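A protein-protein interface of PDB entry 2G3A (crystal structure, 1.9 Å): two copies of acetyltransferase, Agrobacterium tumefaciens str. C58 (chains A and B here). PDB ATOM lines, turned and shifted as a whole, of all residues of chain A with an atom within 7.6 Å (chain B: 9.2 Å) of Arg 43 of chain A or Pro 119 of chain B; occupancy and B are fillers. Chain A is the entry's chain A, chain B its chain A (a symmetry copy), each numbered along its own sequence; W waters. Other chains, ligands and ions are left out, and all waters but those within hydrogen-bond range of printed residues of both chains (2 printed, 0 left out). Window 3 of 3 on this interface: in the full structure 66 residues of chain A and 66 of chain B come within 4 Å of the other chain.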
ATOM      1  N   VAL A  37      24.449  34.139  -5.574  1.00  0.00           N
ATOM      2  CA  VAL A  37      23.731  32.996  -4.988  1.00  0.00           C
ATOM      3  C   VAL A  37      22.229  33.076  -5.308  1.00  0.00           C
ATOM      4  O   VAL A  37      21.626  32.082  -5.712  1.00  0.00           O
ATOM      5  CB  VAL A  37      24.017  32.833  -3.456  1.00  0.00           C
ATOM      6  CG1 VAL A  37      23.218  31.674  -2.860  1.00  0.00           C
ATOM      7  CG2 VAL A  37      25.503  32.610  -3.211  1.00  0.00           C
ATOM      8  N   ALA A  38      21.632  34.259  -5.166  1.00  0.00           N
ATOM      9  CA  ALA A  38      20.200  34.426  -5.451  1.00  0.00           C
ATOM     10  C   ALA A  38      19.885  34.172  -6.924  1.00  0.00           C
ATOM     11  O   ALA A  38      18.886  33.522  -7.252  1.00  0.00           O
ATOM     12  CB  ALA A  38      19.694  35.802  -4.992  1.00  0.00           C
ATOM     13  N   TYR A  39      20.758  34.671  -7.801  1.00  0.00           N
ATOM     14  CA  TYR A  39      20.677  34.423  -9.235  1.00  0.00           C
ATOM     15  C   TYR A  39      20.760  32.932  -9.575  1.00  0.00           C
ATOM     16  O   TYR A  39      20.000  32.437 -10.425  1.00  0.00           O
ATOM     17  CB  TYR A  39      21.792  35.175  -9.978  1.00  0.00           C
ATOM     18  CG  TYR A  39      21.846  34.868 -11.462  1.00  0.00           C
ATOM     19  CD1 TYR A  39      21.114  35.630 -12.378  1.00  0.00           C
ATOM     20  CD2 TYR A  39      22.611  33.809 -11.954  1.00  0.00           C
ATOM     21  CE1 TYR A  39      21.152  35.357 -13.736  1.00  0.00           C
ATOM     22  CE2 TYR A  39      22.657  33.529 -13.322  1.00  0.00           C
ATOM     23  CZ  TYR A  39      21.921  34.304 -14.203  1.00  0.00           C
ATOM     24  OH  TYR A  39      21.943  34.027 -15.555  1.00  0.00           O
ATOM     25  N   ASN A  40      21.706  32.237  -8.943  1.00  0.00           N
ATOM     26  CA  ASN A  40      21.902  30.814  -9.183  1.00  0.00           C
ATOM     27  C   ASN A  40      20.726  29.969  -8.682  1.00  0.00           C
ATOM     28  O   ASN A  40      20.324  29.015  -9.334  1.00  0.00           O
ATOM     29  CB  ASN A  40      23.231  30.336  -8.589  1.00  0.00           C
ATOM     30  CG  ASN A  40      24.424  30.799  -9.392  1.00  0.00           C
ATOM     31  OD1 ASN A  40      24.298  31.179 -10.573  1.00  0.00           O
ATOM     32  ND2 ASN A  40      25.604  30.767  -8.765  1.00  0.00           N
ATOM     33  N   LEU A  41      20.166  30.351  -7.540  1.00  0.00           N
ATOM     34  CA  LEU A  41      18.959  29.713  -7.026  1.00  0.00           C
ATOM     35  C   LEU A  41      17.795  29.848  -8.011  1.00  0.00           C
ATOM     36  O   LEU A  41      17.098  28.868  -8.306  1.00  0.00           O
ATOM     37  CB  LEU A  41      18.576  30.310  -5.668  1.00  0.00           C
ATOM     38  CG  LEU A  41      17.242  29.838  -5.079  1.00  0.00           C
ATOM     39  CD1 LEU A  41      17.312  28.376  -4.681  1.00  0.00           C
ATOM     40  CD2 LEU A  41      16.841  30.710  -3.896  1.00  0.00           C
ATOM     41  N   ALA A  42      17.588  31.064  -8.514  1.00  0.00           N
ATOM     42  CA  ALA A  42      16.465  31.356  -9.405  1.00  0.00           C
ATOM     43  C   ALA A  42      16.611  30.601 -10.719  1.00  0.00           C
ATOM     44  O   ALA A  42      15.632  30.117 -11.275  1.00  0.00           O
ATOM     45  CB  ALA A  42      16.349  32.858  -9.652  1.00  0.00           C
ATOM     46  N   ARG A  43      17.844  30.466 -11.193  1.00  0.00           N
ATOM     47  CA  ARG A  43      18.091  29.854 -12.494  1.00  0.00           C
ATOM     48  C   ARG A  43      18.300  28.329 -12.450  1.00  0.00           C
ATOM     49  O   ARG A  43      17.837  27.600 -13.335  1.00  0.00           O
ATOM     50  CB  ARG A  43      19.295  30.528 -13.152  1.00  0.00           C
ATOM     51  CG  ARG A  43      19.664  29.920 -14.474  1.00  0.00           C
ATOM     52  CD  ARG A  43      20.624  30.776 -15.269  1.00  0.00           C
ATOM     53  NE  ARG A  43      20.911  30.090 -16.529  1.00  0.00           N
ATOM     54  CZ  ARG A  43      21.637  30.584 -17.520  1.00  0.00           C
ATOM     55  NH1 ARG A  43      22.157  31.807 -17.443  1.00  0.00           N
ATOM     56  NH2 ARG A  43      21.819  29.855 -18.612  1.00  0.00           N
ATOM     57  N   PHE A  44      19.008  27.854 -11.432  1.00  0.00           N
ATOM     58  CA  PHE A  44      19.444  26.459 -11.399  1.00  0.00           C
ATOM     59  C   PHE A  44      18.784  25.662 -10.258  1.00  0.00           C
ATOM     60  O   PHE A  44      19.083  24.478 -10.069  1.00  0.00           O
ATOM     61  CB  PHE A  44      20.986  26.380 -11.297  1.00  0.00           C
ATOM     62  CG  PHE A  44      21.724  27.124 -12.390  1.00  0.00           C
ATOM     63  CD1 PHE A  44      21.709  26.666 -13.705  1.00  0.00           C
ATOM     64  CD2 PHE A  44      22.471  28.257 -12.092  1.00  0.00           C
ATOM     65  CE1 PHE A  44      22.399  27.349 -14.712  1.00  0.00           C
ATOM     66  CE2 PHE A  44      23.172  28.943 -13.084  1.00  0.00           C
ATOM     67  CZ  PHE A  44      23.134  28.496 -14.396  1.00  0.00           C
ATOM     68  N   GLY A  45      17.911  26.311  -9.493  1.00  0.00           N
ATOM     69  CA  GLY A  45      17.197  25.658  -8.379  1.00  0.00           C
ATOM     70  C   GLY A  45      18.042  25.525  -7.117  1.00  0.00           C
ATOM     71  O   GLY A  45      19.177  25.989  -7.076  1.00  0.00           O
ATOM     72  N   GLU A  46      17.491  24.869  -6.093  1.00  0.00           N
ATOM     73  CA  GLU A  46      18.164  24.719  -4.795  1.00  0.00           C
ATOM     74  C   GLU A  46      19.514  24.010  -4.904  1.00  0.00           C
ATOM     75  O   GLU A  46      19.653  23.013  -5.623  1.00  0.00           O
ATOM     76  CB  GLU A  46      17.267  23.985  -3.781  1.00  0.00           C
ATOM     77  CG  GLU A  46      16.083  24.797  -3.258  1.00  0.00           C
ATOM     78  CD  GLU A  46      15.197  24.013  -2.277  1.00  0.00           C
ATOM     79  OE1 GLU A  46      15.702  23.110  -1.565  1.00  0.00           O
ATOM     80  OE2 GLU A  46      13.980  24.311  -2.213  1.00  0.00           O
ATOM     81  N   ARG A  73      24.342  20.177  -4.888  1.00  0.00           N
ATOM     82  CA  ARG A  73      23.960  19.777  -6.257  1.00  0.00           C
ATOM     83  C   ARG A  73      24.435  18.352  -6.607  1.00  0.00           C
ATOM     84  O   ARG A  73      24.856  18.061  -7.738  1.00  0.00           O
ATOM     85  CB  ARG A  73      24.456  20.818  -7.272  1.00  0.00           C
ATOM     86  CG  ARG A  73      23.876  22.205  -6.997  1.00  0.00           C
ATOM     87  CD  ARG A  73      24.292  23.260  -8.011  1.00  0.00           C
ATOM     88  NE  ARG A  73      23.707  24.565  -7.688  1.00  0.00           N
ATOM     89  CZ  ARG A  73      22.433  24.888  -7.893  1.00  0.00           C
ATOM     90  NH1 ARG A  73      21.580  24.003  -8.408  1.00  0.00           N
ATOM     91  NH2 ARG A  73      22.003  26.095  -7.552  1.00  0.00           N
ATOM     92  N   ARG B  88      23.705  44.017 -17.850  1.00  0.00           N
ATOM     93  CA  ARG B  88      24.073  42.823 -18.623  1.00  0.00           C
ATOM     94  C   ARG B  88      23.985  43.041 -20.134  1.00  0.00           C
ATOM     95  O   ARG B  88      23.280  43.941 -20.599  1.00  0.00           O
ATOM     96  CB  ARG B  88      23.278  41.599 -18.170  1.00  0.00           C
ATOM     97  CG  ARG B  88      23.740  41.088 -16.814  1.00  0.00           C
ATOM     98  CD  ARG B  88      22.855  39.992 -16.292  1.00  0.00           C
ATOM     99  NE  ARG B  88      22.933  39.935 -14.838  1.00  0.00           N
ATOM    100  CZ  ARG B  88      22.012  39.392 -14.052  1.00  0.00           C
ATOM    101  NH1 ARG B  88      20.915  38.838 -14.567  1.00  0.00           N
ATOM    102  NH2 ARG B  88      22.190  39.416 -12.742  1.00  0.00           N
ATOM    103  N   THR B 116      32.923  27.294 -13.595  1.00  0.00           N
ATOM    104  CA  THR B 116      31.522  27.697 -13.742  1.00  0.00           C
ATOM    105  C   THR B 116      30.592  26.517 -13.993  1.00  0.00           C
ATOM    106  O   THR B 116      31.005  25.509 -14.569  1.00  0.00           O
ATOM    107  CB  THR B 116      31.343  28.755 -14.878  1.00  0.00           C
ATOM    108  OG1 THR B 116      30.020  29.275 -14.826  1.00  0.00           O
ATOM    109  CG2 THR B 116      31.583  28.158 -16.268  1.00  0.00           C
ATOM    110  N   MET B 117      29.342  26.659 -13.564  1.00  0.00           N
ATOM    111  CA  MET B 117      28.273  25.736 -13.964  1.00  0.00           C
ATOM    112  C   MET B 117      27.249  26.396 -14.892  1.00  0.00           C
ATOM    113  O   MET B 117      26.256  25.785 -15.266  1.00  0.00           O
ATOM    114  CB  MET B 117      27.558  25.201 -12.734  1.00  0.00           C
ATOM    115  CG  MET B 117      26.618  26.237 -12.114  1.00  0.00           C
ATOM    116  SD  MET B 117      25.762  25.561 -10.493  1.00  0.00           S
ATOM    117  CE  MET B 117      24.219  24.659 -11.295  1.00  0.00           C
ATOM    118  N   ASN B 118      27.502  27.648 -15.263  1.00  0.00           N
ATOM    119  CA  ASN B 118      26.560  28.457 -16.047  1.00  0.00           C
ATOM    120  C   ASN B 118      27.006  28.507 -17.511  1.00  0.00           C
ATOM    121  O   ASN B 118      28.076  29.046 -17.796  1.00  0.00           O
ATOM    122  CB  ASN B 118      26.523  29.861 -15.425  1.00  0.00           C
ATOM    123  CG  ASN B 118      25.540  30.784 -16.099  1.00  0.00           C
ATOM    124  OD1 ASN B 118      25.254  30.657 -17.278  1.00  0.00           O
ATOM    125  ND2 ASN B 118      25.025  31.732 -15.340  1.00  0.00           N
ATOM    126  N   PRO B 119      26.197  27.948 -18.439  1.00  0.00           N
ATOM    127  CA  PRO B 119      26.567  27.884 -19.851  1.00  0.00           C
ATOM    128  C   PRO B 119      26.800  29.276 -20.468  1.00  0.00           C
ATOM    129  O   PRO B 119      27.620  29.404 -21.375  1.00  0.00           O
ATOM    130  CB  PRO B 119      25.364  27.196 -20.505  1.00  0.00           C
ATOM    131  CG  PRO B 119      24.691  26.501 -19.408  1.00  0.00           C
ATOM    132  CD  PRO B 119      24.874  27.339 -18.209  1.00  0.00           C
ATOM    133  N   ASP B 120      26.113  30.301 -19.956  1.00  0.00           N
ATOM    134  CA  ASP B 120      26.305  31.656 -20.477  1.00  0.00           C
ATOM    135  C   ASP B 120      27.621  32.273 -19.982  1.00  0.00           C
ATOM    136  O   ASP B 120      28.288  32.998 -20.732  1.00  0.00           O
ATOM    137  CB  ASP B 120      25.115  32.553 -20.159  1.00  0.00           C
ATOM    138  CG  ASP B 120      23.845  32.084 -20.850  1.00  0.00           C
ATOM    139  OD1 ASP B 120      23.815  32.009 -22.101  1.00  0.00           O
ATOM    140  OD2 ASP B 120      22.892  31.759 -20.138  1.00  0.00           O
ATOM    141  N   ALA B 121      27.975  31.996 -18.727  1.00  0.00           N
ATOM    142  CA  ALA B 121      29.275  32.399 -18.190  1.00  0.00           C
ATOM    143  C   ALA B 121      30.398  31.673 -18.921  1.00  0.00           C
ATOM    144  O   ALA B 121      31.405  32.293 -19.231  1.00  0.00           O
ATOM    145  CB  ALA B 121      29.364  32.147 -16.702  1.00  0.00           C
ATOM    146  N   LEU B 122      30.221  30.370 -19.186  1.00  0.00           N
ATOM    147  CA  LEU B 122      31.201  29.573 -19.932  1.00  0.00           C
ATOM    148  C   LEU B 122      31.497  30.175 -21.309  1.00  0.00           C
ATOM    149  O   LEU B 122      32.659  30.304 -21.693  1.00  0.00           O
ATOM    150  CB  LEU B 122      30.746  28.105 -20.074  1.00  0.00           C
ATOM    151  CG  LEU B 122      31.625  27.145 -20.905  1.00  0.00           C
ATOM    152  CD1 LEU B 122      33.024  27.047 -20.303  1.00  0.00           C
ATOM    153  CD2 LEU B 122      31.016  25.764 -20.923  1.00  0.00           C
ATOM    154  N   ARG B 123      30.443  30.542 -22.044  1.00  0.00           N
ATOM    155  CA  ARG B 123      30.577  31.202 -23.342  1.00  0.00           C
ATOM    156  C   ARG B 123      31.337  32.531 -23.228  1.00  0.00           C
ATOM    157  O   ARG B 123      32.205  32.831 -24.034  1.00  0.00           O
ATOM    158  CB  ARG B 123      29.187  31.428 -23.945  1.00  0.00           C
ATOM    159  CG  ARG B 123      29.177  31.782 -25.419  1.00  0.00           C
ATOM    160  CD  ARG B 123      27.756  31.987 -25.942  1.00  0.00           C
ATOM    161  NE  ARG B 123      27.016  32.978 -25.163  1.00  0.00           N
ATOM    162  CZ  ARG B 123      26.008  32.691 -24.344  1.00  0.00           C
ATOM    163  NH1 ARG B 123      25.611  31.437 -24.189  1.00  0.00           N
ATOM    164  NH2 ARG B 123      25.403  33.661 -23.674  1.00  0.00           N
ATOM    165  N   THR B 124      30.987  33.329 -22.224  1.00  0.00           N
ATOM    166  CA  THR B 124      31.685  34.590 -21.969  1.00  0.00           C
ATOM    167  C   THR B 124      33.179  34.349 -21.742  1.00  0.00           C
ATOM    168  O   THR B 124      34.032  35.051 -22.315  1.00  0.00           O
ATOM    169  CB  THR B 124      31.089  35.305 -20.730  1.00  0.00           C
ATOM    170  OG1 THR B 124      29.707  35.591 -20.985  1.00  0.00           O
ATOM    171  CG2 THR B 124      31.835  36.611 -20.421  1.00  0.00           C
ATOM    172  N   TYR B 125      33.496  33.351 -20.919  1.00  0.00           N
ATOM    173  CA  TYR B 125      34.902  33.085 -20.580  1.00  0.00           C
ATOM    174  C   TYR B 125      35.659  32.604 -21.787  1.00  0.00           C
ATOM    175  O   TYR B 125      36.798  33.007 -22.009  1.00  0.00           O
ATOM    176  CB  TYR B 125      35.032  32.050 -19.450  1.00  0.00           C
ATOM    177  CG  TYR B 125      34.352  32.443 -18.168  1.00  0.00           C
ATOM    178  CD1 TYR B 125      34.071  33.782 -17.886  1.00  0.00           C
ATOM    179  CD2 TYR B 125      33.984  31.464 -17.221  1.00  0.00           C
ATOM    180  CE1 TYR B 125      33.420  34.140 -16.723  1.00  0.00           C
ATOM    181  CE2 TYR B 125      33.351  31.825 -16.016  1.00  0.00           C
ATOM    182  CZ  TYR B 125      33.069  33.160 -15.787  1.00  0.00           C
ATOM    183  OH  TYR B 125      32.436  33.549 -14.623  1.00  0.00           O
ATOM    184  N   GLU B 126      35.024  31.748 -22.582  1.00  0.00           N
ATOM    185  CA  GLU B 126      35.676  31.245 -23.792  1.00  0.00           C
ATOM    186  C   GLU B 126      35.938  32.350 -24.833  1.00  0.00           C
ATOM    187  O   GLU B 126      37.021  32.404 -25.441  1.00  0.00           O
ATOM    188  CB  GLU B 126      34.874  30.085 -24.378  1.00  0.00           C
ATOM    189  CG  GLU B 126      35.004  28.800 -23.534  1.00  0.00           C
ATOM    190  CD  GLU B 126      34.198  27.627 -24.095  1.00  0.00           C
ATOM    191  OE1 GLU B 126      33.023  27.819 -24.477  1.00  0.00           O
ATOM    192  OE2 GLU B 126      34.734  26.506 -24.128  1.00  0.00           O
ATOM    193  N   ARG B 127      34.952  33.225 -25.029  1.00  0.00           N
ATOM    194  CA  ARG B 127      35.109  34.368 -25.937  1.00  0.00           C
ATOM    195  C   ARG B 127      36.259  35.279 -25.494  1.00  0.00           C
ATOM    196  O   ARG B 127      37.055  35.741 -26.330  1.00  0.00           O
ATOM    197  CB  ARG B 127      33.811  35.176 -26.026  1.00  0.00           C
ATOM    198  CG  ARG B 127      32.740  34.632 -26.959  1.00  0.00           C
ATOM    199  CD  ARG B 127      31.698  35.732 -27.252  1.00  0.00           C
ATOM    200  NE  ARG B 127      30.961  36.104 -26.036  1.00  0.00           N
ATOM    201  CZ  ARG B 127      29.722  35.704 -25.752  1.00  0.00           C
ATOM    202  NH1 ARG B 127      29.051  34.940 -26.610  1.00  0.00           N
ATOM    203  NH2 ARG B 127      29.145  36.083 -24.616  1.00  0.00           N
ATOM    204  N   LYS B 132      39.149  25.489 -21.871  1.00  0.00           N
ATOM    205  CA  LYS B 132      38.698  24.481 -20.933  1.00  0.00           C
ATOM    206  C   LYS B 132      39.830  23.549 -20.570  1.00  0.00           C
ATOM    207  O   LYS B 132      40.619  23.147 -21.422  1.00  0.00           O
ATOM    208  CB  LYS B 132      37.541  23.685 -21.544  1.00  0.00           C
ATOM    209  CG  LYS B 132      36.359  24.561 -21.933  1.00  0.00           C
ATOM    210  CD  LYS B 132      35.048  23.787 -22.033  1.00  0.00           C
ATOM    211  CE  LYS B 132      34.710  23.421 -23.469  1.00  0.00           C
ATOM    212  NZ  LYS B 132      33.229  23.337 -23.655  1.00  0.00           N
ATOM    213  N   SER B 141      21.154  18.937 -10.610  1.00  0.00           N
ATOM    214  CA  SER B 141      20.269  19.829 -11.321  1.00  0.00           C
ATOM    215  C   SER B 141      20.461  19.804 -12.846  1.00  0.00           C
ATOM    216  O   SER B 141      19.733  20.496 -13.568  1.00  0.00           O
ATOM    217  CB  SER B 141      20.360  21.240 -10.737  1.00  0.00           C
ATOM    218  OG  SER B 141      21.668  21.516 -10.256  1.00  0.00           O
ATOM    219  N   GLY B 142      21.435  19.014 -13.318  1.00  0.00           N
ATOM    220  CA  GLY B 142      21.659  18.774 -14.749  1.00  0.00           C
ATOM    221  C   GLY B 142      22.786  19.506 -15.450  1.00  0.00           C
ATOM    222  O   GLY B 142      23.125  19.179 -16.584  1.00  0.00           O
ATOM    223  N   GLN B 143      23.364  20.500 -14.789  1.00  0.00           N
ATOM    224  CA  GLN B 143      24.459  21.277 -15.336  1.00  0.00           C
ATOM    225  C   GLN B 143      25.769  20.528 -15.120  1.00  0.00           C
ATOM    226  O   GLN B 143      25.792  19.461 -14.505  1.00  0.00           O
ATOM    227  CB  GLN B 143      24.545  22.641 -14.628  1.00  0.00           C
ATOM    228  CG  GLN B 143      23.248  23.445 -14.645  1.00  0.00           C
ATOM    229  CD  GLN B 143      22.238  22.955 -13.626  1.00  0.00           C
ATOM    230  OE1 GLN B 143      22.579  22.215 -12.676  1.00  0.00           O
ATOM    231  NE2 GLN B 143      20.973  23.339 -13.828  1.00  0.00           N
ATOM    232  N   SER B 144      26.843  21.072 -15.680  1.00  0.00           N
ATOM    233  CA  SER B 144      28.183  20.560 -15.435  1.00  0.00           C
ATOM    234  C   SER B 144      29.048  21.649 -14.815  1.00  0.00           C
ATOM    235  O   SER B 144      28.736  22.848 -14.925  1.00  0.00           O
ATOM    236  CB  SER B 144      28.815  20.069 -16.745  1.00  0.00           C
ATOM    237  OG  SER B 144      29.011  21.143 -17.644  1.00  0.00           O
ATOM    238  N   ILE B 145      30.126  21.243 -14.148  1.00  0.00           N
ATOM    239  CA  ILE B 145      31.185  22.195 -13.764  1.00  0.00           C
ATOM    240  C   ILE B 145      32.300  22.145 -14.814  1.00  0.00           C
ATOM    241  O   ILE B 145      32.711  21.058 -15.230  1.00  0.00           O
ATOM    242  CB  ILE B 145      31.770  21.934 -12.352  1.00  0.00           C
ATOM    243  CG1 ILE B 145      30.648  21.872 -11.306  1.00  0.00           C
ATOM    244  CG2 ILE B 145      32.826  23.024 -11.989  1.00  0.00           C
ATOM    245  CD1 ILE B 145      31.099  21.587  -9.861  1.00  0.00           C
ATOM    246  N   THR B 146      32.764  23.316 -15.267  1.00  0.00           N
ATOM    247  CA  THR B 146      33.882  23.384 -16.221  1.00  0.00           C
ATOM    248  C   THR B 146      34.963  24.265 -15.620  1.00  0.00           C
ATOM    249  O   THR B 146      34.648  25.313 -15.032  1.00  0.00           O
ATOM    250  CB  THR B 146      33.440  23.966 -17.597  1.00  0.00           C
ATOM    251  OG1 THR B 146      32.319  23.227 -18.078  1.00  0.00           O
ATOM    252  CG2 THR B 146      34.588  23.877 -18.649  1.00  0.00           C
ATOM    253  N   LEU B 148      38.545  26.317 -16.510  1.00  0.00           N
ATOM    254  CA  LEU B 148      39.215  26.905 -17.659  1.00  0.00           C
ATOM    255  C   LEU B 148      40.492  27.623 -17.237  1.00  0.00           C
ATOM    256  O   LEU B 148      40.587  28.098 -16.104  1.00  0.00           O
ATOM    257  CB  LEU B 148      38.276  27.914 -18.382  1.00  0.00           C
ATOM    258  CG  LEU B 148      36.946  27.366 -18.896  1.00  0.00           C
ATOM    259  CD1 LEU B 148      35.840  27.641 -17.896  1.00  0.00           C
ATOM    260  CD2 LEU B 148      36.575  27.977 -20.260  1.00  0.00           C
HETATM  261  O   HOH W   1      22.307  29.241 -21.757  1.00  0.00           O
HETATM  262  O   HOH W   2      25.923  31.618 -12.433  1.00  0.00           O
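NH1 of Arg 73 of chain A sits at hydrogen-bond distance from OG of Ser 141 of chain B (3.1 Å).
NH2 of Arg 43 of chain A is in salt-bridge range of OD2 of Asp 120 of chain B, 2.7 Å away.
SD of Met 117 of chain B lies within hydrogen-bond range of NE of Arg 73 of chain A (3.6 Å).
The side-chain amide oxygen (OD1) of Asn 118 of chain B sits at hydrogen-bond distance from the guanidinium group (NH1) of Arg 43 of chain A, at 3.3 Å.
The side-chain hydroxyl of Tyr 39 of chain A is in hydrogen-bond range of the guanidinium group of Arg 43 of chain A (2.9 Å).
The side-chain amide oxygen (OD1) of Asn 118 of chain B sits at hydrogen-bond distance from the backbone NH (N) of Asp 120 of chain B, at 2.8 Å.
The backbone carbonyl oxygen of Phe 44 of chain A is in hydrogen-bond range of the guanidinium group of Arg 73 of chain A, 3.0 Å away.
OG1 of Thr 124 of chain B lies within hydrogen-bond range of O of Asp 120 of chain B, at 3.0 Å.
The guanidinium group (NH2) of Arg 73 of chain A is in hydrogen-bond range of the backbone carbonyl oxygen (O) of Gly 45 of chain A, 2.9 Å away.
The side-chain amide oxygen (OD1) of Asn 118 of chain B is in hydrogen-bond range of the backbone NH (N) of Ala 121 of chain B, 3.4 Å away.
NH1 of Arg 88 of chain B touches CE1 of Tyr 39 of chain A, at 3.6 Å.
Tyr 39 of chain A touches Asn 118 of chain B (CE2 to ND2, 3.6 Å).
CD of Pro 119 of chain B touches NH2 of Arg 43 of chain A (3.98 Å).
CB of Phe 44 of chain A touches CE of Met 117 of chain B, at 3.7 Å.
CZ of Phe 44 of chain A touches CG of Asn 118 of chain B (3.7 Å).
Phe 44 of chain A touches Ser 141 of chain B.
Gln 143 of chain B touches Phe 44 of chain A.
Printed residues of chain B within 4 Å of Tyr 39 of chain A: Arg 88 and Asn 118.
No residue of chain B comes within 4 Å of Ala 42 of chain A.
Of chain B, only Asn 118 (3.3 Å), Pro 119 (3.98 Å) and Asp 120 (2.7 Å) come within 4 Å of Arg 43 of chain A.
Of chain B, only Met 117 (3.7 Å), Asn 118 (3.7 Å), Ser 141 (3.5 Å) and Gln 143 (3.4 Å) come within 4 Å of Phe 44 of chain A.
Of the printed residues of chain B, Arg 73 of chain A touches Met 117 and Ser 141.
Printed residues of chain A within 4 Å of Arg 88 of chain B: Tyr 39.
Printed residues of chain A within 4 Å of Asn 118 of chain B: Tyr 39 (3.6 Å), Arg 43 (3.3 Å) and Phe 44 (3.7 Å).
Of chain A, only Arg 43 comes within 4 Å of Pro 119 of chain B.
Tyr 125 of chain B touches none of the printed residues of chain A.
The nearest residue of chain B that does not touch Arg 43 of chain A is Gln 143 of chain B (5.3 Å).
The nearest printed residue of chain A that does not touch Arg 88 of chain B is Arg 43 of chain A (7.7 Å).
Hydrophobic or aromatic side chains of chain B that line the printed part of chain A: Met 117 and Pro 119.
Of the 11 printed residues of chain A, 4 touch a printed residue of chain B.
Printed residues of chain A that touch a printed residue of chain B: Tyr 39, Arg 43, Phe 44 and Arg 73.
Hydrophobic or aromatic side chains of chain A within 4 Å of the printed part of chain B: Tyr 39 and Phe 44.
Along chain A the printed residues that touch a printed residue of chain B span positions 39 to 73.
Among the printed residues, Asp or Glu carboxylates within 4 Å of a Lys or Arg side-chain nitrogen of the other chain: Arg 43 of chain A with Asp 120 of chain B (2.7 Å).
No position is printed for both chains.
Of the 11 pairs that touch across the chains among the printed residues, none has its exchanged pair printed and touching as well.
Water W2 bridges OD1 of Asn 40 of chain A (2.5 Å) and ND2 of Asn 118 of chain B (3.0 Å).
Water W1 bridges OD2 of Asp 120 of chain B and NH2 of Arg 43 of chain A.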
